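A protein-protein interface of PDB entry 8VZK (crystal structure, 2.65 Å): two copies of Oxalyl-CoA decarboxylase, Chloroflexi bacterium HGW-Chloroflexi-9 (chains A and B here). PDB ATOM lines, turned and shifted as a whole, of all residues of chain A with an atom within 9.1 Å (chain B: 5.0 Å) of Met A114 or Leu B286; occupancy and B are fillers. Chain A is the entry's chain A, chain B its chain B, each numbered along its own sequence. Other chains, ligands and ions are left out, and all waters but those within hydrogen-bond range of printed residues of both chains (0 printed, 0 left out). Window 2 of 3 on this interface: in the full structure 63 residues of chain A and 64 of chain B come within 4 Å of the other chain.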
ATOM      1  N   TYR A 107     -24.382 -12.613 -22.035  1.00  0.00           N
ATOM      2  CA  TYR A 107     -23.724 -13.503 -21.091  1.00  0.00           C
ATOM      3  C   TYR A 107     -24.730 -14.470 -20.480  1.00  0.00           C
ATOM      4  O   TYR A 107     -25.904 -14.143 -20.287  1.00  0.00           O
ATOM      5  CB  TYR A 107     -23.035 -12.695 -19.990  1.00  0.00           C
ATOM      6  CG  TYR A 107     -23.967 -11.779 -19.226  1.00  0.00           C
ATOM      7  CD1 TYR A 107     -24.199 -10.479 -19.656  1.00  0.00           C
ATOM      8  CD2 TYR A 107     -24.617 -12.214 -18.076  1.00  0.00           C
ATOM      9  CE1 TYR A 107     -25.051  -9.638 -18.965  1.00  0.00           C
ATOM     10  CE2 TYR A 107     -25.472 -11.380 -17.379  1.00  0.00           C
ATOM     11  CZ  TYR A 107     -25.685 -10.092 -17.827  1.00  0.00           C
ATOM     12  OH  TYR A 107     -26.533  -9.258 -17.137  1.00  0.00           O
ATOM     13  N   GLU A 108     -24.259 -15.677 -20.181  1.00  0.00           N
ATOM     14  CA  GLU A 108     -25.106 -16.664 -19.530  1.00  0.00           C
ATOM     15  C   GLU A 108     -25.458 -16.211 -18.117  1.00  0.00           C
ATOM     16  O   GLU A 108     -24.686 -15.514 -17.453  1.00  0.00           O
ATOM     17  CB  GLU A 108     -24.407 -18.022 -19.488  1.00  0.00           C
ATOM     18  CG  GLU A 108     -24.021 -18.557 -20.855  1.00  0.00           C
ATOM     19  CD  GLU A 108     -23.343 -19.908 -20.783  1.00  0.00           C
ATOM     20  OE1 GLU A 108     -23.071 -20.380 -19.658  1.00  0.00           O
ATOM     21  OE2 GLU A 108     -23.082 -20.500 -21.851  1.00  0.00           O
ATOM     22  N   GLN A 109     -26.649 -16.608 -17.662  1.00  0.00           N
ATOM     23  CA  GLN A 109     -27.086 -16.228 -16.322  1.00  0.00           C
ATOM     24  C   GLN A 109     -26.178 -16.827 -15.257  1.00  0.00           C
ATOM     25  O   GLN A 109     -25.913 -16.194 -14.228  1.00  0.00           O
ATOM     26  CB  GLN A 109     -28.535 -16.657 -16.097  1.00  0.00           C
ATOM     27  CG  GLN A 109     -29.540 -15.969 -17.005  1.00  0.00           C
ATOM     28  CD  GLN A 109     -30.974 -16.327 -16.662  1.00  0.00           C
ATOM     29  OE1 GLN A 109     -31.240 -17.379 -16.082  1.00  0.00           O
ATOM     30  NE2 GLN A 109     -31.903 -15.446 -17.014  1.00  0.00           N
ATOM     31  N   THR A 110     -25.685 -18.044 -15.488  1.00  0.00           N
ATOM     32  CA  THR A 110     -24.786 -18.690 -14.540  1.00  0.00           C
ATOM     33  C   THR A 110     -23.383 -18.098 -14.559  1.00  0.00           C
ATOM     34  O   THR A 110     -22.556 -18.488 -13.727  1.00  0.00           O
ATOM     35  CB  THR A 110     -24.708 -20.190 -14.828  1.00  0.00           C
ATOM     36  OG1 THR A 110     -24.071 -20.403 -16.095  1.00  0.00           O
ATOM     37  CG2 THR A 110     -26.103 -20.796 -14.863  1.00  0.00           C
ATOM     38  N   GLY A 111     -23.094 -17.180 -15.477  1.00  0.00           N
ATOM     39  CA  GLY A 111     -21.778 -16.579 -15.559  1.00  0.00           C
ATOM     40  C   GLY A 111     -21.792 -15.080 -15.336  1.00  0.00           C
ATOM     41  O   GLY A 111     -20.822 -14.388 -15.662  1.00  0.00           O
ATOM     42  N   HIS A 112     -22.889 -14.571 -14.781  1.00  0.00           N
ATOM     43  CA  HIS A 112     -23.000 -13.143 -14.514  1.00  0.00           C
ATOM     44  C   HIS A 112     -21.969 -12.716 -13.477  1.00  0.00           C
ATOM     45  O   HIS A 112     -21.720 -13.423 -12.497  1.00  0.00           O
ATOM     46  CB  HIS A 112     -24.413 -12.809 -14.029  1.00  0.00           C
ATOM     47  CG  HIS A 112     -24.720 -11.343 -14.010  1.00  0.00           C
ATOM     48  ND1 HIS A 112     -23.948 -10.410 -14.670  1.00  0.00           N
ATOM     49  CD2 HIS A 112     -25.718 -10.649 -13.414  1.00  0.00           C
ATOM     50  CE1 HIS A 112     -24.458  -9.206 -14.479  1.00  0.00           C
ATOM     51  NE2 HIS A 112     -25.532  -9.324 -13.720  1.00  0.00           N
ATOM     52  N   LEU A 113     -21.356 -11.553 -13.712  1.00  0.00           N
ATOM     53  CA  LEU A 113     -20.368 -10.966 -12.805  1.00  0.00           C
ATOM     54  C   LEU A 113     -19.131 -11.847 -12.651  1.00  0.00           C
ATOM     55  O   LEU A 113     -18.449 -11.803 -11.623  1.00  0.00           O
ATOM     56  CB  LEU A 113     -20.979 -10.665 -11.432  1.00  0.00           C
ATOM     57  CG  LEU A 113     -22.203  -9.750 -11.419  1.00  0.00           C
ATOM     58  CD1 LEU A 113     -22.660  -9.513  -9.992  1.00  0.00           C
ATOM     59  CD2 LEU A 113     -21.898  -8.435 -12.118  1.00  0.00           C
ATOM     60  N   MET A 114     -18.824 -12.652 -13.667  1.00  0.00           N
ATOM     61  CA  MET A 114     -17.627 -13.480 -13.661  1.00  0.00           C
ATOM     62  C   MET A 114     -16.586 -13.047 -14.682  1.00  0.00           C
ATOM     63  O   MET A 114     -15.493 -13.621 -14.703  1.00  0.00           O
ATOM     64  CB  MET A 114     -17.986 -14.950 -13.926  1.00  0.00           C
ATOM     65  CG  MET A 114     -18.899 -15.578 -12.897  1.00  0.00           C
ATOM     66  SD  MET A 114     -19.120 -17.339 -13.211  1.00  0.00           S
ATOM     67  CE  MET A 114     -17.432 -17.917 -13.070  1.00  0.00           C
ATOM     68  N   GLY A 115     -16.888 -12.061 -15.518  1.00  0.00           N
ATOM     69  CA  GLY A 115     -16.035 -11.775 -16.652  1.00  0.00           C
ATOM     70  C   GLY A 115     -16.296 -12.693 -17.825  1.00  0.00           C
ATOM     71  O   GLY A 115     -15.355 -13.085 -18.527  1.00  0.00           O
ATOM     72  N   PHE A 116     -17.557 -13.054 -18.050  1.00  0.00           N
ATOM     73  CA  PHE A 116     -17.918 -13.982 -19.112  1.00  0.00           C
ATOM     74  C   PHE A 116     -17.570 -13.394 -20.476  1.00  0.00           C
ATOM     75  O   PHE A 116     -17.366 -12.187 -20.633  1.00  0.00           O
ATOM     76  CB  PHE A 116     -19.410 -14.315 -19.031  1.00  0.00           C
ATOM     77  CG  PHE A 116     -19.826 -15.480 -19.888  1.00  0.00           C
ATOM     78  CD1 PHE A 116     -19.556 -16.780 -19.493  1.00  0.00           C
ATOM     79  CD2 PHE A 116     -20.500 -15.274 -21.082  1.00  0.00           C
ATOM     80  CE1 PHE A 116     -19.941 -17.853 -20.279  1.00  0.00           C
ATOM     81  CE2 PHE A 116     -20.886 -16.342 -21.871  1.00  0.00           C
ATOM     82  CZ  PHE A 116     -20.607 -17.633 -21.469  1.00  0.00           C
ATOM     83  N   PHE A 117     -17.490 -14.273 -21.473  1.00  0.00           N
ATOM     84  CA  PHE A 117     -17.142 -13.857 -22.826  1.00  0.00           C
ATOM     85  C   PHE A 117     -18.184 -12.890 -23.371  1.00  0.00           C
ATOM     86  O   PHE A 117     -19.368 -13.230 -23.471  1.00  0.00           O
ATOM     87  CB  PHE A 117     -17.017 -15.080 -23.733  1.00  0.00           C
ATOM     88  CG  PHE A 117     -16.663 -14.747 -25.155  1.00  0.00           C
ATOM     89  CD1 PHE A 117     -15.436 -14.184 -25.465  1.00  0.00           C
ATOM     90  CD2 PHE A 117     -17.553 -15.011 -26.183  1.00  0.00           C
ATOM     91  CE1 PHE A 117     -15.107 -13.879 -26.774  1.00  0.00           C
ATOM     92  CE2 PHE A 117     -17.229 -14.711 -27.494  1.00  0.00           C
ATOM     93  CZ  PHE A 117     -16.004 -14.143 -27.789  1.00  0.00           C
ATOM     94  N   GLU A 119     -19.425 -10.366 -21.981  1.00  0.00           N
ATOM     95  CA  GLU A 119     -20.355  -9.901 -20.961  1.00  0.00           C
ATOM     96  C   GLU A 119     -20.309  -8.380 -20.891  1.00  0.00           C
ATOM     97  O   GLU A 119     -19.244  -7.796 -20.667  1.00  0.00           O
ATOM     98  CB  GLU A 119     -20.004 -10.514 -19.607  1.00  0.00           C
ATOM     99  CG  GLU A 119     -20.839  -9.993 -18.451  1.00  0.00           C
ATOM    100  CD  GLU A 119     -20.393 -10.555 -17.114  1.00  0.00           C
ATOM    101  OE1 GLU A 119     -19.448 -11.373 -17.098  1.00  0.00           O
ATOM    102  OE2 GLU A 119     -20.985 -10.178 -16.080  1.00  0.00           O
ATOM    103  N   LEU B 278      -9.082 -13.180 -14.114  1.00  0.00           N
ATOM    104  CA  LEU B 278      -9.642 -14.531 -14.175  1.00  0.00           C
ATOM    105  C   LEU B 278     -10.998 -14.477 -14.880  1.00  0.00           C
ATOM    106  O   LEU B 278     -12.059 -14.723 -14.300  1.00  0.00           O
ATOM    107  CB  LEU B 278      -9.759 -15.131 -12.782  1.00  0.00           C
ATOM    108  CG  LEU B 278      -8.476 -15.685 -12.163  1.00  0.00           C
ATOM    109  CD1 LEU B 278      -8.779 -16.345 -10.831  1.00  0.00           C
ATOM    110  CD2 LEU B 278      -7.808 -16.669 -13.111  1.00  0.00           C
ATOM    111  N   ASN B 279     -10.944 -14.141 -16.162  1.00  0.00           N
ATOM    112  CA  ASN B 279     -12.126 -14.006 -16.991  1.00  0.00           C
ATOM    113  C   ASN B 279     -12.320 -15.281 -17.815  1.00  0.00           C
ATOM    114  O   ASN B 279     -11.808 -16.350 -17.462  1.00  0.00           O
ATOM    115  CB  ASN B 279     -11.991 -12.749 -17.861  1.00  0.00           C
ATOM    116  CG  ASN B 279     -10.648 -12.667 -18.570  1.00  0.00           C
ATOM    117  OD1 ASN B 279      -9.927 -13.658 -18.685  1.00  0.00           O
ATOM    118  ND2 ASN B 279     -10.310 -11.475 -19.050  1.00  0.00           N
ATOM    119  N   HIS B 283     -10.420 -19.069 -17.956  1.00  0.00           N
ATOM    120  CA  HIS B 283     -11.375 -20.079 -17.488  1.00  0.00           C
ATOM    121  C   HIS B 283     -11.842 -19.817 -16.058  1.00  0.00           C
ATOM    122  O   HIS B 283     -12.153 -20.752 -15.313  1.00  0.00           O
ATOM    123  CB  HIS B 283     -10.785 -21.486 -17.609  1.00  0.00           C
ATOM    124  CG  HIS B 283     -10.181 -21.770 -18.946  1.00  0.00           C
ATOM    125  ND1 HIS B 283     -10.923 -21.793 -20.107  1.00  0.00           N
ATOM    126  CD2 HIS B 283      -8.903 -22.032 -19.311  1.00  0.00           C
ATOM    127  CE1 HIS B 283     -10.130 -22.063 -21.128  1.00  0.00           C
ATOM    128  NE2 HIS B 283      -8.899 -22.212 -20.671  1.00  0.00           N
ATOM    129  N   PHE B 284     -11.883 -18.543 -15.668  1.00  0.00           N
ATOM    130  CA  PHE B 284     -12.314 -18.080 -14.350  1.00  0.00           C
ATOM    131  C   PHE B 284     -11.510 -18.691 -13.204  1.00  0.00           C
ATOM    132  O   PHE B 284     -11.918 -18.584 -12.043  1.00  0.00           O
ATOM    133  CB  PHE B 284     -13.812 -18.336 -14.135  1.00  0.00           C
ATOM    134  CG  PHE B 284     -14.659 -17.991 -15.329  1.00  0.00           C
ATOM    135  CD1 PHE B 284     -14.971 -16.673 -15.621  1.00  0.00           C
ATOM    136  CD2 PHE B 284     -15.141 -18.988 -16.163  1.00  0.00           C
ATOM    137  CE1 PHE B 284     -15.747 -16.356 -16.721  1.00  0.00           C
ATOM    138  CE2 PHE B 284     -15.916 -18.678 -17.263  1.00  0.00           C
ATOM    139  CZ  PHE B 284     -16.220 -17.360 -17.543  1.00  0.00           C
ATOM    140  N   GLY B 285     -10.373 -19.323 -13.495  1.00  0.00           N
ATOM    141  CA  GLY B 285      -9.606 -19.995 -12.460  1.00  0.00           C
ATOM    142  C   GLY B 285     -10.326 -21.142 -11.787  1.00  0.00           C
ATOM    143  O   GLY B 285      -9.911 -21.578 -10.710  1.00  0.00           O
ATOM    144  N   LEU B 286     -11.388 -21.651 -12.395  1.00  0.00           N
ATOM    145  CA  LEU B 286     -12.244 -22.659 -11.795  1.00  0.00           C
ATOM    146  C   LEU B 286     -12.034 -24.021 -12.443  1.00  0.00           C
ATOM    147  O   LEU B 286     -11.552 -24.117 -13.576  1.00  0.00           O
ATOM    148  CB  LEU B 286     -13.718 -22.250 -11.929  1.00  0.00           C
ATOM    149  CG  LEU B 286     -14.153 -20.993 -11.172  1.00  0.00           C
ATOM    150  CD1 LEU B 286     -15.629 -20.716 -11.404  1.00  0.00           C
ATOM    151  CD2 LEU B 286     -13.858 -21.132  -9.686  1.00  0.00           C
ATOM    152  N   PRO B 287     -12.371 -25.100 -11.740  1.00  0.00           N
ATOM    153  CA  PRO B 287     -12.323 -26.434 -12.348  1.00  0.00           C
ATOM    154  C   PRO B 287     -13.285 -26.533 -13.519  1.00  0.00           C
ATOM    155  O   PRO B 287     -14.226 -25.732 -13.627  1.00  0.00           O
ATOM    156  CB  PRO B 287     -12.748 -27.360 -11.196  1.00  0.00           C
ATOM    157  CG  PRO B 287     -12.411 -26.601  -9.965  1.00  0.00           C
ATOM    158  CD  PRO B 287     -12.660 -25.162 -10.298  1.00  0.00           C
ATOM    159  N   PRO B 288     -13.092 -27.509 -14.420  1.00  0.00           N
ATOM    160  CA  PRO B 288     -12.059 -28.556 -14.425  1.00  0.00           C
ATOM    161  C   PRO B 288     -10.723 -28.069 -14.975  1.00  0.00           C
ATOM    162  O   PRO B 288      -9.724 -28.780 -14.910  1.00  0.00           O
ATOM    163  CB  PRO B 288     -12.683 -29.632 -15.319  1.00  0.00           C
ATOM    164  CG  PRO B 288     -13.460 -28.838 -16.328  1.00  0.00           C
ATOM    165  CD  PRO B 288     -14.014 -27.656 -15.562  1.00  0.00           C
ATOM    166  N   ARG B 289     -10.680 -26.854 -15.524  1.00  0.00           N
ATOM    167  CA  ARG B 289      -9.435 -26.333 -16.078  1.00  0.00           C
ATOM    168  C   ARG B 289      -8.417 -25.998 -14.997  1.00  0.00           C
ATOM    169  O   ARG B 289      -7.232 -25.840 -15.308  1.00  0.00           O
ATOM    170  CB  ARG B 289      -9.721 -25.090 -16.925  1.00  0.00           C
ATOM    171  CG  ARG B 289     -11.042 -25.144 -17.682  1.00  0.00           C
ATOM    172  CD  ARG B 289     -11.025 -26.168 -18.807  1.00  0.00           C
ATOM    173  NE  ARG B 289     -10.496 -25.616 -20.049  1.00  0.00           N
ATOM    174  CZ  ARG B 289      -9.261 -25.808 -20.493  1.00  0.00           C
ATOM    175  NH1 ARG B 289      -8.392 -26.546 -19.821  1.00  0.00           N
ATOM    176  NH2 ARG B 289      -8.890 -25.250 -21.642  1.00  0.00           N
ATOM    177  N   PHE B 290      -8.847 -25.886 -13.742  1.00  0.00           N
ATOM    178  CA  PHE B 290      -7.972 -25.535 -12.633  1.00  0.00           C
ATOM    179  C   PHE B 290      -8.239 -26.456 -11.453  1.00  0.00           C
ATOM    180  O   PHE B 290      -9.305 -27.066 -11.338  1.00  0.00           O
ATOM    181  CB  PHE B 290      -8.168 -24.075 -12.197  1.00  0.00           C
ATOM    182  CG  PHE B 290      -7.661 -23.069 -13.188  1.00  0.00           C
ATOM    183  CD1 PHE B 290      -8.375 -22.788 -14.339  1.00  0.00           C
ATOM    184  CD2 PHE B 290      -6.475 -22.391 -12.959  1.00  0.00           C
ATOM    185  CE1 PHE B 290      -7.911 -21.865 -15.251  1.00  0.00           C
ATOM    186  CE2 PHE B 290      -6.007 -21.461 -13.867  1.00  0.00           C
ATOM    187  CZ  PHE B 290      -6.727 -21.197 -15.014  1.00  0.00           C
ATOM    188  N   ILE B 308     -11.726 -11.918  -7.588  1.00  0.00           N
ATOM    189  CA  ILE B 308     -12.807 -12.235  -8.515  1.00  0.00           C
ATOM    190  C   ILE B 308     -12.762 -13.716  -8.866  1.00  0.00           C
ATOM    191  O   ILE B 308     -11.695 -14.265  -9.174  1.00  0.00           O
ATOM    192  CB  ILE B 308     -12.712 -11.361  -9.774  1.00  0.00           C
ATOM    193  CG1 ILE B 308     -12.899  -9.888  -9.414  1.00  0.00           C
ATOM    194  CG2 ILE B 308     -13.751 -11.790 -10.802  1.00  0.00           C
ATOM    195  CD1 ILE B 308     -14.173  -9.612  -8.656  1.00  0.00           C
ATOM    196  N   ASN B 309     -13.925 -14.371  -8.803  1.00  0.00           N
ATOM    197  CA  ASN B 309     -14.111 -15.772  -9.177  1.00  0.00           C
ATOM    198  C   ASN B 309     -13.394 -16.739  -8.238  1.00  0.00           C
ATOM    199  O   ASN B 309     -14.003 -17.698  -7.756  1.00  0.00           O
ATOM    200  CB  ASN B 309     -13.662 -16.018 -10.621  1.00  0.00           C
ATOM    201  CG  ASN B 309     -14.623 -15.435 -11.638  1.00  0.00           C
ATOM    202  OD1 ASN B 309     -15.822 -15.325 -11.383  1.00  0.00           O
ATOM    203  ND2 ASN B 309     -14.101 -15.065 -12.800  1.00  0.00           N
ATOM    204  N   VAL B 310     -12.110 -16.512  -7.978  1.00  0.00           N
ATOM    205  CA  VAL B 310     -11.308 -17.364  -7.109  1.00  0.00           C
ATOM    206  C   VAL B 310     -10.719 -16.488  -6.012  1.00  0.00           C
ATOM    207  O   VAL B 310     -10.211 -15.405  -6.309  1.00  0.00           O
ATOM    208  CB  VAL B 310     -10.188 -18.096  -7.871  1.00  0.00           C
ATOM    209  CG1 VAL B 310      -9.354 -18.941  -6.921  1.00  0.00           C
ATOM    210  CG2 VAL B 310     -10.777 -18.962  -8.974  1.00  0.00           C
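The side-chain amide nitrogen of Asn B309 sits at hydrogen-bond distance from the backbone carbonyl oxygen of Met A114, at 2.8 Å.
N of Gly A115 is in hydrogen-bond range of OE1 of Glu A119. The backbone NH of Phe A116 is in hydrogen-bond range of the side-chain carboxylate of Glu A119. ND2 of Asn B309 lies within hydrogen-bond range of O of Leu B278 (2.6 Å). The backbone carbonyl oxygen (O) of Asn B279 sits at hydrogen-bond distance from the backbone NH (N) of Phe B284, at 2.8 Å.
Among the printed residues, pairs that only touch across the chains: Met A114 with Leu B278, Met A114 with Phe B284, Met A114 with Leu B286, Gly A115 with Asn B279, Gly A115 with Phe B284 and Phe A116 with Phe B284.
Of chain B, only Leu B278, Phe B284, Leu B286 and Asn B309 come within 4 Å of Met A114. Leu B286 touches just one residue of chain A: Met A114 (3.7 Å). Of the printed residues of chain A, Phe B284 touches Met A114, Gly A115 and Phe A116. No residue of chain A comes within 4 Å of Gly B285. Of the printed residues of chain A, Asn B279 touches Gly A115 (3.4 Å). Printed residues of chain B within 4 Å of Gly A115: Asn B279 (3.4 Å) and Phe B284 (3.8 Å). Of the printed residues of chain A, Leu B278 touches Met A114 (3.6 Å). Of the printed residues of chain A, Asn B309 touches Met A114. His A112 touches none of the printed residues of chain B. The nearest printed residue of chain B that does not touch Gly A115 is Asn B309 (4.9 Å).
Of the 13 printed residues of chain B, 5 touch a printed residue of chain A. Hydrophobic or aromatic side chains of chain A that line the printed part of chain B: Met A114 and Phe A116. Among the printed residues, no Asp or Glu carboxylate lies within 4 Å of a Lys or Arg side-chain nitrogen of the other chain.
No position is printed for both chains.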
